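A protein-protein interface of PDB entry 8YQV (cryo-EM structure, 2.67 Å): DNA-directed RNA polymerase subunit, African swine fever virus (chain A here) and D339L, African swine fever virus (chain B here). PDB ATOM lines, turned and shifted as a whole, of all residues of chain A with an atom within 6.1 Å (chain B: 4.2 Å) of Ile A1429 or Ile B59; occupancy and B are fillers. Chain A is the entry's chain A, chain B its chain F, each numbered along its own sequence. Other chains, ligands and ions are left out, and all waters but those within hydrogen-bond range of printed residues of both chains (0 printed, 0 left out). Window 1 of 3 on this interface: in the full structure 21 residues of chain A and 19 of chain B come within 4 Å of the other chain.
N of Arg B61 is in hydrogen-bond range of OH of Tyr A5 (3.2 Å). The backbone carbonyl oxygen of Ile A1429 sits at hydrogen-bond distance from the backbone NH of Ile B59, at 3.1 Å. The backbone NH (N) of Met A1431 lies within hydrogen-bond range of the backbone carbonyl oxygen (O) of Cys B57, at 3.2 Å.
The backbone NH of Tyr B69 lies within hydrogen-bond range of the backbone carbonyl oxygen of Phe B58 (2.8 Å). The backbone NH of Met B60 lies within hydrogen-bond range of the backbone carbonyl oxygen of Arg B67 (2.8 Å).
Among the printed residues, pairs that only touch across the chains: Tyr A5 with Tyr B69 (3.4 Å), Ile A1430 with Phe B58 (3.4 Å), Ile A1430 with Cys B57 (3.5 Å), Met A1431 with Ile B59 (3.6 Å), Asp A1428 with Phe B58 (3.7 Å), Ile A1429 with Phe B58 (3.7 Å), Tyr A5 with Met B60 (3.9 Å) and Asp A1428 with Ile B59 (3.96 Å).
Printed residues of chain B within 4 Å of Tyr A5: Met B60 (3.9 Å), Arg B61 (3.2 Å) and Tyr B69 (3.4 Å). Of chain B, only Phe B58 and Ile B59 come within 4 Å of Ile A1429. Of the printed residues of chain B, Ile A1430 touches Cys B57 and Phe B58. Of the printed residues of chain A, Phe B58 touches Asp A1428, Ile A1429 and Ile A1430. Ile B59 touches three residues of chain A. Of the printed residues of chain A, Arg B61 touches Tyr A5. The nearest printed residue of chain A that does not touch Phe B58 is Met A1431 (5.2 Å).
Hydrophobic or aromatic side chains of chain B within 4 Å of the printed part of chain A: Phe B58, Ile B59, Met B60 and Tyr B69. Hydrophobic or aromatic side chains of chain A that line the printed part of chain B: Tyr A5, Ile A1429, Ile A1430 and Met A1431. Among the printed residues, no Asp or Glu carboxylate lies within 4 Å of a Lys or Arg side-chain nitrogen of the other chain.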
ATOM      1  N   TYR A   5       7.852   7.301   7.336  1.00  0.00           N
ATOM      2  CA  TYR A   5       9.179   7.552   6.797  1.00  0.00           C
ATOM      3  C   TYR A   5       9.858   6.246   6.411  1.00  0.00           C
ATOM      4  O   TYR A   5       9.886   5.294   7.195  1.00  0.00           O
ATOM      5  CB  TYR A   5      10.021   8.297   7.829  1.00  0.00           C
ATOM      6  CG  TYR A   5      11.463   8.496   7.442  1.00  0.00           C
ATOM      7  CD1 TYR A   5      11.846   9.550   6.644  1.00  0.00           C
ATOM      8  CD2 TYR A   5      12.439   7.627   7.881  1.00  0.00           C
ATOM      9  CE1 TYR A   5      13.157   9.730   6.298  1.00  0.00           C
ATOM     10  CE2 TYR A   5      13.748   7.797   7.538  1.00  0.00           C
ATOM     11  CZ  TYR A   5      14.103   8.848   6.749  1.00  0.00           C
ATOM     12  OH  TYR A   5      15.420   9.016   6.407  1.00  0.00           O
ATOM     13  N   MET A 472      20.784  22.552  10.860  1.00  0.00           N
ATOM     14  CA  MET A 472      21.684  21.406  10.782  1.00  0.00           C
ATOM     15  C   MET A 472      22.863  21.673   9.863  1.00  0.00           C
ATOM     16  O   MET A 472      23.993  21.294  10.178  1.00  0.00           O
ATOM     17  CB  MET A 472      20.940  20.163  10.312  1.00  0.00           C
ATOM     18  CG  MET A 472      19.839  19.697  11.210  1.00  0.00           C
ATOM     19  SD  MET A 472      19.692  17.921  11.030  1.00  0.00           S
ATOM     20  CE  MET A 472      18.195  17.620  11.924  1.00  0.00           C
ATOM     21  N   SER A1427      26.259   7.051  11.893  1.00  0.00           N
ATOM     22  CA  SER A1427      25.613   6.569  13.103  1.00  0.00           C
ATOM     23  C   SER A1427      24.195   7.110  13.195  1.00  0.00           C
ATOM     24  O   SER A1427      23.930   8.258  12.834  1.00  0.00           O
ATOM     25  CB  SER A1427      26.401   6.979  14.346  1.00  0.00           C
ATOM     26  OG  SER A1427      27.631   6.289  14.420  1.00  0.00           O
ATOM     27  N   ASP A1428      23.288   6.271  13.674  1.00  0.00           N
ATOM     28  CA  ASP A1428      21.892   6.640  13.836  1.00  0.00           C
ATOM     29  C   ASP A1428      21.689   7.254  15.211  1.00  0.00           C
ATOM     30  O   ASP A1428      22.288   6.814  16.193  1.00  0.00           O
ATOM     31  CB  ASP A1428      20.988   5.420  13.665  1.00  0.00           C
ATOM     32  CG  ASP A1428      19.603   5.782  13.166  1.00  0.00           C
ATOM     33  OD1 ASP A1428      19.227   6.971  13.230  1.00  0.00           O
ATOM     34  OD2 ASP A1428      18.883   4.872  12.706  1.00  0.00           O
ATOM     35  N   ILE A1429      20.849   8.278  15.275  1.00  0.00           N
ATOM     36  CA  ILE A1429      20.489   8.928  16.526  1.00  0.00           C
ATOM     37  C   ILE A1429      19.094   8.468  16.912  1.00  0.00           C
ATOM     38  O   ILE A1429      18.198   8.400  16.065  1.00  0.00           O
ATOM     39  CB  ILE A1429      20.552  10.460  16.401  1.00  0.00           C
ATOM     40  CG1 ILE A1429      21.905  10.908  15.850  1.00  0.00           C
ATOM     41  CG2 ILE A1429      20.289  11.111  17.730  1.00  0.00           C
ATOM     42  CD1 ILE A1429      23.088  10.494  16.683  1.00  0.00           C
ATOM     43  N   ILE A1430      18.917   8.113  18.177  1.00  0.00           N
ATOM     44  CA  ILE A1430      17.611   7.802  18.735  1.00  0.00           C
ATOM     45  C   ILE A1430      17.403   8.691  19.948  1.00  0.00           C
ATOM     46  O   ILE A1430      18.353   9.194  20.548  1.00  0.00           O
ATOM     47  CB  ILE A1430      17.467   6.315  19.110  1.00  0.00           C
ATOM     48  CG1 ILE A1430      18.412   5.952  20.247  1.00  0.00           C
ATOM     49  CG2 ILE A1430      17.753   5.443  17.925  1.00  0.00           C
ATOM     50  CD1 ILE A1430      18.212   4.572  20.761  1.00  0.00           C
ATOM     51  N   MET A1431      16.142   8.894  20.304  1.00  0.00           N
ATOM     52  CA  MET A1431      15.795   9.806  21.381  1.00  0.00           C
ATOM     53  C   MET A1431      15.880   9.073  22.711  1.00  0.00           C
ATOM     54  O   MET A1431      15.363   7.959  22.846  1.00  0.00           O
ATOM     55  CB  MET A1431      14.391  10.371  21.170  1.00  0.00           C
ATOM     56  CG  MET A1431      14.252  11.210  19.914  1.00  0.00           C
ATOM     57  SD  MET A1431      14.672  12.947  20.054  1.00  0.00           S
ATOM     58  CE  MET A1431      14.507  13.200  21.803  1.00  0.00           C
ATOM     59  N   CYS B  57      12.562   5.872  18.973  1.00  0.00           N
ATOM     60  CA  CYS B  57      12.210   7.022  18.146  1.00  0.00           C
ATOM     61  C   CYS B  57      13.454   7.442  17.375  1.00  0.00           C
ATOM     62  O   CYS B  57      14.266   8.234  17.844  1.00  0.00           O
ATOM     63  CB  CYS B  57      11.663   8.158  18.999  1.00  0.00           C
ATOM     64  SG  CYS B  57      11.093   9.581  18.046  1.00  0.00           S
ATOM     65  N   PHE B  58      13.614   6.886  16.181  1.00  0.00           N
ATOM     66  CA  PHE B  58      14.730   7.250  15.327  1.00  0.00           C
ATOM     67  C   PHE B  58      14.543   8.656  14.783  1.00  0.00           C
ATOM     68  O   PHE B  58      13.426   9.100  14.527  1.00  0.00           O
ATOM     69  CB  PHE B  58      14.861   6.279  14.157  1.00  0.00           C
ATOM     70  CG  PHE B  58      14.965   4.846  14.560  1.00  0.00           C
ATOM     71  CD1 PHE B  58      16.135   4.349  15.090  1.00  0.00           C
ATOM     72  CD2 PHE B  58      13.900   3.989  14.386  1.00  0.00           C
ATOM     73  CE1 PHE B  58      16.237   3.032  15.454  1.00  0.00           C
ATOM     74  CE2 PHE B  58      14.001   2.668  14.745  1.00  0.00           C
ATOM     75  CZ  PHE B  58      15.172   2.191  15.281  1.00  0.00           C
ATOM     76  N   ILE B  59      15.644   9.344  14.592  1.00  0.00           N
ATOM     77  CA  ILE B  59      15.639  10.662  13.973  1.00  0.00           C
ATOM     78  C   ILE B  59      15.800  10.485  12.475  1.00  0.00           C
ATOM     79  O   ILE B  59      16.693   9.766  12.020  1.00  0.00           O
ATOM     80  CB  ILE B  59      16.753  11.545  14.560  1.00  0.00           C
ATOM     81  CG1 ILE B  59      16.674  11.552  16.081  1.00  0.00           C
ATOM     82  CG2 ILE B  59      16.650  12.948  14.030  1.00  0.00           C
ATOM     83  CD1 ILE B  59      15.365  12.022  16.610  1.00  0.00           C
ATOM     84  N   MET B  60      14.925  11.122  11.702  1.00  0.00           N
ATOM     85  CA  MET B  60      14.946  10.949  10.257  1.00  0.00           C
ATOM     86  C   MET B  60      16.259  11.448   9.679  1.00  0.00           C
ATOM     87  O   MET B  60      16.751  12.520  10.033  1.00  0.00           O
ATOM     88  CB  MET B  60      13.760  11.662   9.614  1.00  0.00           C
ATOM     89  CG  MET B  60      12.443  11.332  10.289  1.00  0.00           C
ATOM     90  SD  MET B  60      10.962  12.028   9.540  1.00  0.00           S
ATOM     91  CE  MET B  60      11.698  13.190   8.419  1.00  0.00           C
ATOM     92  N   ARG B  61      16.826  10.652   8.779  1.00  0.00           N
ATOM     93  CA  ARG B  61      18.207  10.802   8.358  1.00  0.00           C
ATOM     94  C   ARG B  61      18.363  11.463   6.999  1.00  0.00           C
ATOM     95  O   ARG B  61      19.418  12.035   6.729  1.00  0.00           O
ATOM     96  CB  ARG B  61      18.874   9.425   8.325  1.00  0.00           C
ATOM     97  CG  ARG B  61      20.362   9.429   8.173  1.00  0.00           C
ATOM     98  CD  ARG B  61      20.834   8.156   7.509  1.00  0.00           C
ATOM     99  NE  ARG B  61      21.327   8.399   6.160  1.00  0.00           N
ATOM    100  CZ  ARG B  61      20.860   7.811   5.069  1.00  0.00           C
ATOM    101  NH1 ARG B  61      19.885   6.921   5.129  1.00  0.00           N
ATOM    102  NH2 ARG B  61      21.384   8.124   3.890  1.00  0.00           N
ATOM    103  N   ARG B  67      13.048  15.628  12.691  1.00  0.00           N
ATOM    104  CA  ARG B  67      11.822  14.942  13.052  1.00  0.00           C
ATOM    105  C   ARG B  67      12.116  13.474  13.318  1.00  0.00           C
ATOM    106  O   ARG B  67      13.166  12.954  12.940  1.00  0.00           O
ATOM    107  CB  ARG B  67      10.788  15.082  11.937  1.00  0.00           C
ATOM    108  CG  ARG B  67       9.840  16.239  12.124  1.00  0.00           C
ATOM    109  CD  ARG B  67       8.780  16.246  11.050  1.00  0.00           C
ATOM    110  NE  ARG B  67       9.350  16.065   9.723  1.00  0.00           N
ATOM    111  CZ  ARG B  67       8.718  15.492   8.709  1.00  0.00           C
ATOM    112  NH1 ARG B  67       7.492  15.016   8.841  1.00  0.00           N
ATOM    113  NH2 ARG B  67       9.333  15.387   7.536  1.00  0.00           N
ATOM    114  N   TYR B  69      10.764   9.168  13.745  1.00  0.00           N
ATOM    115  CA  TYR B  69       9.839   8.164  13.253  1.00  0.00           C
ATOM    116  C   TYR B  69       9.950   6.934  14.133  1.00  0.00           C
ATOM    117  O   TYR B  69      10.985   6.676  14.745  1.00  0.00           O
ATOM    118  CB  TYR B  69      10.089   7.825  11.780  1.00  0.00           C
ATOM    119  CG  TYR B  69      11.396   7.133  11.482  1.00  0.00           C
ATOM    120  CD1 TYR B  69      12.553   7.859  11.259  1.00  0.00           C
ATOM    121  CD2 TYR B  69      11.467   5.757  11.401  1.00  0.00           C
ATOM    122  CE1 TYR B  69      13.739   7.232  10.975  1.00  0.00           C
ATOM    123  CE2 TYR B  69      12.649   5.125  11.121  1.00  0.00           C
ATOM    124  CZ  TYR B  69      13.780   5.868  10.907  1.00  0.00           C
ATOM    125  OH  TYR B  69      14.961   5.236  10.623  1.00  0.00           O
